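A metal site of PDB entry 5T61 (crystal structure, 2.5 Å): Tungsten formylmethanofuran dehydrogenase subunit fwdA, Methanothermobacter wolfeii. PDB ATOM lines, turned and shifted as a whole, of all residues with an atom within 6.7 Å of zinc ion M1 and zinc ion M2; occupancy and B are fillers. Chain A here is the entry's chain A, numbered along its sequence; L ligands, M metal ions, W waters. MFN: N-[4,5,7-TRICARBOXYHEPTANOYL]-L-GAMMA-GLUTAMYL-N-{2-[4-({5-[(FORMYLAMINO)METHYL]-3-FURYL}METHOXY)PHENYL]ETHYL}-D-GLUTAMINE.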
ATOM      1  N   HIS A  57     -10.265  -3.072  30.550  1.00  0.00           N
ATOM      2  CA  HIS A  57      -9.178  -2.581  29.694  1.00  0.00           C
ATOM      3  C   HIS A  57      -8.379  -3.777  29.178  1.00  0.00           C
ATOM      4  O   HIS A  57      -7.575  -4.360  29.916  1.00  0.00           O
ATOM      5  CB  HIS A  57      -8.288  -1.611  30.458  1.00  0.00           C
ATOM      6  CG  HIS A  57      -7.353  -0.844  29.568  1.00  0.00           C
ATOM      7  ND1 HIS A  57      -7.534   0.484  29.273  1.00  0.00           N
ATOM      8  CD2 HIS A  57      -6.261  -1.241  28.868  1.00  0.00           C
ATOM      9  CE1 HIS A  57      -6.580   0.893  28.461  1.00  0.00           C
ATOM     10  NE2 HIS A  57      -5.790  -0.133  28.198  1.00  0.00           N
ATOM     11  N   SER A  58      -8.599  -4.107  27.907  1.00  0.00           N
ATOM     12  CA  SER A  58      -7.881  -5.190  27.254  1.00  0.00           C
ATOM     13  C   SER A  58      -7.838  -4.899  25.761  1.00  0.00           C
ATOM     14  O   SER A  58      -8.657  -4.136  25.233  1.00  0.00           O
ATOM     15  CB  SER A  58      -8.548  -6.544  27.535  1.00  0.00           C
ATOM     16  OG  SER A  58      -7.709  -7.614  27.125  1.00  0.00           O
ATOM     17  N   HIS A  59      -6.865  -5.497  25.083  1.00  0.00           N
ATOM     18  CA  HIS A  59      -6.701  -5.377  23.635  1.00  0.00           C
ATOM     19  C   HIS A  59      -6.952  -6.751  23.020  1.00  0.00           C
ATOM     20  O   HIS A  59      -6.078  -7.619  23.035  1.00  0.00           O
ATOM     21  CB  HIS A  59      -5.320  -4.821  23.323  1.00  0.00           C
ATOM     22  CG  HIS A  59      -5.111  -3.431  23.844  1.00  0.00           C
ATOM     23  ND1 HIS A  59      -4.350  -3.151  24.952  1.00  0.00           N
ATOM     24  CD2 HIS A  59      -5.570  -2.236  23.393  1.00  0.00           C
ATOM     25  CE1 HIS A  59      -4.354  -1.842  25.176  1.00  0.00           C
ATOM     26  NE2 HIS A  59      -5.090  -1.266  24.241  1.00  0.00           N
ATOM     27  N   ALA A 115      -9.973  -1.593  24.453  1.00  0.00           N
ATOM     28  CA  ALA A 115      -9.615  -0.296  25.017  1.00  0.00           C
ATOM     29  C   ALA A 115      -9.108   0.724  23.999  1.00  0.00           C
ATOM     30  O   ALA A 115      -8.881   1.879  24.386  1.00  0.00           O
ATOM     31  CB  ALA A 115      -8.566  -0.476  26.111  1.00  0.00           C
ATOM     32  N   ALA A 116      -8.900   0.353  22.731  1.00  0.00           N
ATOM     33  CA  ALA A 116      -8.351   1.317  21.774  1.00  0.00           C
ATOM     34  C   ALA A 116      -8.781   0.929  20.368  1.00  0.00           C
ATOM     35  O   ALA A 116      -8.171   0.057  19.742  1.00  0.00           O
ATOM     36  CB  ALA A 116      -6.832   1.380  21.892  1.00  0.00           C
ATOM     37  N   KCX A 178     -11.824   7.370  24.859  1.00  0.00           N
ATOM     38  CA  KCX A 178     -10.447   6.919  25.218  1.00  0.00           C
ATOM     39  CB  KCX A 178     -10.158   5.559  24.590  1.00  0.00           C
ATOM     40  CG  KCX A 178      -8.733   5.042  24.830  1.00  0.00           C
ATOM     41  CD  KCX A 178      -8.502   4.557  26.259  1.00  0.00           C
ATOM     42  CE  KCX A 178      -7.026   4.227  26.461  1.00  0.00           C
ATOM     43  NZ  KCX A 178      -6.585   3.037  25.757  1.00  0.00           N
ATOM     44  C   KCX A 178      -9.458   7.961  24.771  1.00  0.00           C
ATOM     45  O   KCX A 178      -9.647   8.600  23.706  1.00  0.00           O
ATOM     46  CX  KCX A 178      -5.387   2.484  25.955  1.00  0.00           C
ATOM     47  OQ1 KCX A 178      -4.547   2.985  26.672  1.00  0.00           O
ATOM     48  OQ2 KCX A 178      -5.080   1.342  25.344  1.00  0.00           O
ATOM     49  N   ILE A 179      -8.427   8.181  25.580  1.00  0.00           N
ATOM     50  CA  ILE A 179      -7.391   9.174  25.296  1.00  0.00           C
ATOM     51  C   ILE A 179      -6.023   8.533  25.535  1.00  0.00           C
ATOM     52  O   ILE A 179      -5.721   8.121  26.651  1.00  0.00           O
ATOM     53  CB  ILE A 179      -7.559  10.425  26.177  1.00  0.00           C
ATOM     54  CG1 ILE A 179      -8.963  11.012  26.050  1.00  0.00           C
ATOM     55  CG2 ILE A 179      -6.494  11.458  25.824  1.00  0.00           C
ATOM     56  CD1 ILE A 179      -9.278  12.057  27.114  1.00  0.00           C
ATOM     57  N   VAL A 180      -5.190   8.477  24.495  1.00  0.00           N
ATOM     58  CA  VAL A 180      -3.855   7.897  24.595  1.00  0.00           C
ATOM     59  C   VAL A 180      -2.845   8.945  24.145  1.00  0.00           C
ATOM     60  O   VAL A 180      -2.907   9.410  23.002  1.00  0.00           O
ATOM     61  CB  VAL A 180      -3.711   6.620  23.743  1.00  0.00           C
ATOM     62  CG1 VAL A 180      -2.268   6.128  23.779  1.00  0.00           C
ATOM     63  CG2 VAL A 180      -4.658   5.554  24.226  1.00  0.00           C
ATOM     64  N   HIS A 231      -4.845   7.454  29.135  1.00  0.00           N
ATOM     65  CA  HIS A 231      -3.493   6.919  29.017  1.00  0.00           C
ATOM     66  C   HIS A 231      -2.573   8.125  28.897  1.00  0.00           C
ATOM     67  O   HIS A 231      -2.627   8.861  27.905  1.00  0.00           O
ATOM     68  CB  HIS A 231      -3.448   5.977  27.807  1.00  0.00           C
ATOM     69  CG  HIS A 231      -2.072   5.599  27.340  1.00  0.00           C
ATOM     70  ND1 HIS A 231      -1.752   4.314  26.972  1.00  0.00           N
ATOM     71  CD2 HIS A 231      -0.970   6.349  27.083  1.00  0.00           C
ATOM     72  CE1 HIS A 231      -0.493   4.266  26.563  1.00  0.00           C
ATOM     73  NE2 HIS A 231       0.001   5.484  26.619  1.00  0.00           N
ATOM     74  N   LEU A 235       4.589   8.078  28.901  1.00  0.00           N
ATOM     75  CA  LEU A 235       4.525   6.698  29.381  1.00  0.00           C
ATOM     76  C   LEU A 235       5.894   6.039  29.372  1.00  0.00           C
ATOM     77  O   LEU A 235       6.657   6.169  28.408  1.00  0.00           O
ATOM     78  CB  LEU A 235       3.545   5.856  28.545  1.00  0.00           C
ATOM     79  CG  LEU A 235       3.441   4.386  29.023  1.00  0.00           C
ATOM     80  CD1 LEU A 235       2.026   3.878  28.841  1.00  0.00           C
ATOM     81  CD2 LEU A 235       4.414   3.403  28.294  1.00  0.00           C
ATOM     82  N   THR A 270      -5.630   4.469  33.367  1.00  0.00           N
ATOM     83  CA  THR A 270      -5.363   3.067  33.079  1.00  0.00           C
ATOM     84  C   THR A 270      -3.865   2.781  33.109  1.00  0.00           C
ATOM     85  O   THR A 270      -3.042   3.673  32.911  1.00  0.00           O
ATOM     86  CB  THR A 270      -5.963   2.660  31.724  1.00  0.00           C
ATOM     87  OG1 THR A 270      -5.747   1.264  31.491  1.00  0.00           O
ATOM     88  CG2 THR A 270      -5.363   3.480  30.604  1.00  0.00           C
ATOM     89  N   HIS A 271      -3.544   1.506  33.358  1.00  0.00           N
ATOM     90  CA  HIS A 271      -2.201   0.974  33.543  1.00  0.00           C
ATOM     91  C   HIS A 271      -1.252   1.995  34.158  1.00  0.00           C
ATOM     92  O   HIS A 271      -0.208   2.320  33.581  1.00  0.00           O
ATOM     93  CB  HIS A 271      -1.632   0.447  32.225  1.00  0.00           C
ATOM     94  CG  HIS A 271      -1.800   1.381  31.062  1.00  0.00           C
ATOM     95  ND1 HIS A 271      -1.168   2.605  30.994  1.00  0.00           N
ATOM     96  CD2 HIS A 271      -2.516   1.256  29.912  1.00  0.00           C
ATOM     97  CE1 HIS A 271      -1.504   3.206  29.860  1.00  0.00           C
ATOM     98  NE2 HIS A 271      -2.310   2.412  29.194  1.00  0.00           N
ATOM     99  N   HIS A 275       2.995   4.703  34.578  1.00  0.00           N
ATOM    100  CA  HIS A 275       3.039   6.147  34.759  1.00  0.00           C
ATOM    101  C   HIS A 275       3.538   6.530  36.157  1.00  0.00           C
ATOM    102  O   HIS A 275       3.324   7.660  36.590  1.00  0.00           O
ATOM    103  CB  HIS A 275       1.658   6.756  34.508  1.00  0.00           C
ATOM    104  CG  HIS A 275       1.084   6.425  33.165  1.00  0.00           C
ATOM    105  ND1 HIS A 275       1.512   7.017  31.996  1.00  0.00           N
ATOM    106  CD2 HIS A 275       0.094   5.577  32.812  1.00  0.00           C
ATOM    107  CE1 HIS A 275       0.822   6.543  30.979  1.00  0.00           C
ATOM    108  NE2 HIS A 275      -0.047   5.657  31.444  1.00  0.00           N
ATOM    109  N   MET A 317       1.263  -3.511  22.403  1.00  0.00           N
ATOM    110  CA  MET A 317       0.465  -2.951  21.330  1.00  0.00           C
ATOM    111  C   MET A 317      -0.344  -1.791  21.892  1.00  0.00           C
ATOM    112  O   MET A 317      -1.158  -1.970  22.797  1.00  0.00           O
ATOM    113  CB  MET A 317      -0.463  -4.019  20.730  1.00  0.00           C
ATOM    114  CG  MET A 317      -1.237  -4.851  21.748  1.00  0.00           C
ATOM    115  SD  MET A 317      -2.295  -6.082  20.983  1.00  0.00           S
ATOM    116  CE  MET A 317      -1.103  -7.137  20.168  1.00  0.00           C
ATOM    117  N   THR A 318      -0.125  -0.590  21.340  1.00  0.00           N
ATOM    118  CA  THR A 318      -0.704   0.619  21.916  1.00  0.00           C
ATOM    119  C   THR A 318      -0.985   1.580  20.776  1.00  0.00           C
ATOM    120  O   THR A 318      -0.415   1.450  19.684  1.00  0.00           O
ATOM    121  CB  THR A 318       0.234   1.259  22.927  1.00  0.00           C
ATOM    122  OG1 THR A 318      -0.406   2.391  23.549  1.00  0.00           O
ATOM    123  CG2 THR A 318       1.445   1.759  22.205  1.00  0.00           C
ATOM    124  N   ALA A 319      -1.871   2.534  21.035  1.00  0.00           N
ATOM    125  CA  ALA A 319      -2.031   3.691  20.169  1.00  0.00           C
ATOM    126  C   ALA A 319      -0.953   4.749  20.401  1.00  0.00           C
ATOM    127  O   ALA A 319      -0.991   5.807  19.775  1.00  0.00           O
ATOM    128  CB  ALA A 319      -3.419   4.306  20.374  1.00  0.00           C
ATOM    129  N   ASP A 320       0.000   4.467  21.291  1.00  0.00           N
ATOM    130  CA  ASP A 320       1.113   5.355  21.586  1.00  0.00           C
ATOM    131  C   ASP A 320       2.284   5.017  20.676  1.00  0.00           C
ATOM    132  O   ASP A 320       3.304   4.456  21.083  1.00  0.00           O
ATOM    133  CB  ASP A 320       1.474   5.233  23.068  1.00  0.00           C
ATOM    134  CG  ASP A 320       2.228   6.432  23.602  1.00  0.00           C
ATOM    135  OD1 ASP A 320       2.935   7.103  22.830  1.00  0.00           O
ATOM    136  OD2 ASP A 320       2.085   6.687  24.814  1.00  0.00           O
ATOM    137  N   ASP A 385      -3.083  -4.487  31.349  1.00  0.00           N
ATOM    138  CA  ASP A 385      -3.192  -3.829  30.042  1.00  0.00           C
ATOM    139  C   ASP A 385      -2.997  -4.846  28.920  1.00  0.00           C
ATOM    140  O   ASP A 385      -2.245  -4.637  27.969  1.00  0.00           O
ATOM    141  CB  ASP A 385      -2.206  -2.671  29.931  1.00  0.00           C
ATOM    142  CG  ASP A 385      -2.428  -1.846  28.681  1.00  0.00           C
ATOM    143  OD1 ASP A 385      -3.532  -1.918  28.096  1.00  0.00           O
ATOM    144  OD2 ASP A 385      -1.508  -1.127  28.269  1.00  0.00           O
ATOM    145  N   SER A 386      -3.687  -5.974  29.066  1.00  0.00           N
ATOM    146  CA  SER A 386      -3.433  -7.169  28.279  1.00  0.00           C
ATOM    147  C   SER A 386      -3.404  -6.882  26.784  1.00  0.00           C
ATOM    148  O   SER A 386      -4.314  -6.250  26.253  1.00  0.00           O
ATOM    149  CB  SER A 386      -4.495  -8.230  28.573  1.00  0.00           C
ATOM    150  OG  SER A 386      -4.217  -9.425  27.879  1.00  0.00           O
ATOM    151  N   ASN A 388      -0.110  -5.930  27.142  1.00  0.00           N
ATOM    152  CA  ASN A 388       1.072  -5.069  27.253  1.00  0.00           C
ATOM    153  C   ASN A 388       1.926  -5.419  28.450  1.00  0.00           C
ATOM    154  O   ASN A 388       3.156  -5.490  28.359  1.00  0.00           O
ATOM    155  CB  ASN A 388       0.674  -3.592  27.333  1.00  0.00           C
ATOM    156  CG  ASN A 388       0.171  -3.028  26.024  1.00  0.00           C
ATOM    157  OD1 ASN A 388       0.924  -2.890  25.066  1.00  0.00           O
ATOM    158  ND2 ASN A 388      -1.089  -2.621  26.010  1.00  0.00           N
HETATM  159  C1  MFN L   1       0.458   1.101  27.558  1.00  0.00           C
HETATM  160  O1  MFN L   1       2.095   0.030  25.912  1.00  0.00           O
HETATM  161  C2  MFN L   1       1.754   0.384  27.159  1.00  0.00           C
HETATM  162  O2  MFN L   1       5.820  -0.110  28.385  1.00  0.00           O
HETATM  163  C3  MFN L   1       2.765   0.000  28.081  1.00  0.00           C
HETATM  164  O3  MFN L   1      15.016  -0.696  30.598  1.00  0.00           O
HETATM  165  C4  MFN L   1       3.736  -0.623  27.299  1.00  0.00           C
HETATM  166  O4  MFN L   1      19.269   0.427  28.602  1.00  0.00           O
HETATM  167  C5  MFN L   1       3.305  -0.586  25.976  1.00  0.00           C
HETATM  168  O5  MFN L   1      18.874  -1.575  27.847  1.00  0.00           O
HETATM  169  C6  MFN L   1       9.990  -0.852  29.268  1.00  0.00           C
HETATM  170  N3  MFN L   1      19.172  -1.160  30.990  1.00  0.00           N
HETATM  171  C21 MFN L   1      19.082  -1.028  32.440  1.00  0.00           C
HETATM  172  O6  MFN L   1      18.037  -0.800  33.018  1.00  0.00           O
HETATM  173  C22 MFN L   1      20.389  -1.167  33.199  1.00  0.00           C
HETATM  174  C14 MFN L   1      20.412  -2.144  34.387  1.00  0.00           C
HETATM  175  C23 MFN L   1      21.853  -2.517  34.687  1.00  0.00           C
HETATM  176  C24 MFN L   1      22.769  -1.311  34.950  1.00  0.00           C
HETATM  177  O7  MFN L   1      23.306  -1.193  36.084  1.00  0.00           O
HETATM  178  O8  MFN L   1      23.050  -0.428  34.076  1.00  0.00           O
HETATM  179  N4  MFN L   1      21.890  -3.307  35.873  1.00  0.00           N
HETATM  180  C25 MFN L   1      23.019  -4.155  36.152  1.00  0.00           C
HETATM  181  O9  MFN L   1      23.940  -4.195  35.364  1.00  0.00           O
HETATM  182  C26 MFN L   1      23.085  -4.996  37.455  1.00  0.00           C
HETATM  183  C27 MFN L   1      24.156  -4.335  38.416  1.00  0.00           C
HETATM  184  C28 MFN L   1      23.841  -4.723  39.888  1.00  0.00           C
HETATM  185  C29 MFN L   1      24.198  -6.163  40.092  1.00  0.00           C
HETATM  186  O10 MFN L   1      23.322  -6.994  40.474  1.00  0.00           O
HETATM  187  O11 MFN L   1      25.390  -6.553  39.898  1.00  0.00           O
HETATM  188  C19 MFN L   1      18.084  -1.037  30.057  1.00  0.00           C
HETATM  189  C20 MFN L   1      18.763  -0.713  28.761  1.00  0.00           C
HETATM  190  C16 MFN L   1      14.876  -1.245  29.532  1.00  0.00           C
HETATM  191  C17 MFN L   1      16.032  -2.114  28.938  1.00  0.00           C
HETATM  192  C18 MFN L   1      17.201  -2.316  29.945  1.00  0.00           C
HETATM  193  N2  MFN L   1      13.629  -1.084  28.781  1.00  0.00           N
HETATM  194  C15 MFN L   1      12.523  -0.281  29.277  1.00  0.00           C
HETATM  195  C12 MFN L   1      11.348  -1.165  29.854  1.00  0.00           C
HETATM  196  C11 MFN L   1       9.465   0.391  29.402  1.00  0.00           C
HETATM  197  C10 MFN L   1       8.144   0.659  29.059  1.00  0.00           C
HETATM  198  C7  MFN L   1       9.111  -1.883  29.145  1.00  0.00           C
HETATM  199  C8  MFN L   1       7.801  -1.658  28.691  1.00  0.00           C
HETATM  200  C9  MFN L   1       7.167  -0.365  28.771  1.00  0.00           C
HETATM  201  C13 MFN L   1       5.077  -1.223  27.825  1.00  0.00           C
HETATM  202  N1  MFN L   1      -0.545   0.939  26.536  1.00  0.00           N
HETATM  203  O12 MFN L   1      25.917  -3.953  45.112  1.00  0.00           O
HETATM  204  C30 MFN L   1      25.303  -4.829  44.449  1.00  0.00           C
HETATM  205  O13 MFN L   1      24.556  -5.643  45.032  1.00  0.00           O
HETATM  206  C31 MFN L   1      25.473  -4.880  42.964  1.00  0.00           C
HETATM  207  C32 MFN L   1      24.267  -4.181  42.271  1.00  0.00           C
HETATM  208  C33 MFN L   1      24.632  -3.835  40.842  1.00  0.00           C
HETATM  209  C34 MFN L   1      24.329  -2.392  40.591  1.00  0.00           C
HETATM  210  O14 MFN L   1      25.220  -1.635  40.111  1.00  0.00           O
HETATM  211  O15 MFN L   1      23.188  -1.944  40.866  1.00  0.00           O
HETATM  212 ZN    ZN M   1      -2.708   2.327  27.004  1.00  0.00          ZN
HETATM  213 ZN    ZN M   2      -4.239  -0.394  26.763  1.00  0.00          ZN
HETATM  214  O   HOH W   1      -3.345   2.099  23.789  1.00  0.00           O
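The side-chain carboxylate (OD2) of Asp 385 is in salt-bridge range of a nitrogen (N1) of the ligand (2.9 Å). The side-chain amide oxygen of Asn 388 sits close to an oxygen (O1) of the ligand, at 3.3 Å. N1 of the ligand is in hydrogen-bond range of OG1 of Thr 318.
OQ2 of KCX 178 sits close to a ring nitrogen (NE2) of His 59, at 2.8 Å. A ring nitrogen (ND1) of His 57 lies within hydrogen-bond range of the side-chain hydroxyl (OG1) of Thr 270 (3.0 Å). The side-chain amide nitrogen of Asn 388 sits at hydrogen-bond distance from the side-chain carboxylate of Asp 385 (2.7 Å). A ring nitrogen (ND1) of His 59 lies close to the side-chain amide nitrogen (ND2) of Asn 388, at 3.5 Å. The backbone NH of His 59 is in hydrogen-bond range of the backbone carbonyl oxygen of Ser 386, at 2.9 Å. A ring nitrogen (NE2) of His 231 is in hydrogen-bond range of the side-chain carboxylate of Asp 320 (3.0 Å). O of Ile 179 is in hydrogen-bond range of N of His 231. The side-chain amide oxygen (OD1) of Asn 388 sits at hydrogen-bond distance from the backbone NH (N) of Met 317 (2.8 Å).
Within 4 Å of zinc ion M1: KCX 178, His 231, His 271 and Asp 385.
Merely in contact with zinc ion M2: Asn 388.
Zinc ion M1 is bound by OQ1 of KCX 178 (2.0 Å), ND1 of His 231 (2.2 Å) and NE2 of His 271 (2.2 Å). Zinc ion M1 has three donor atoms within binding distance. Slightly farther from zinc ion M1 lies a nitrogen (N1) of the ligand (2.6 Å).
Zinc ion M2 is bound by a ring nitrogen (NE2) of His 57 (2.1 Å), the side-chain carboxylate of Asp 385 (2.1 Å) and OQ2 of KCX 178 (2.4 Å). Slightly farther from zinc ion M2 lies NE2 of His 59 (2.8 Å).
Water W1 lies within hydrogen-bond range of the side-chain hydroxyl (OG1) of Thr 318 (3.0 Å) and the backbone NH (N) of Ala 319 (3.2 Å).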
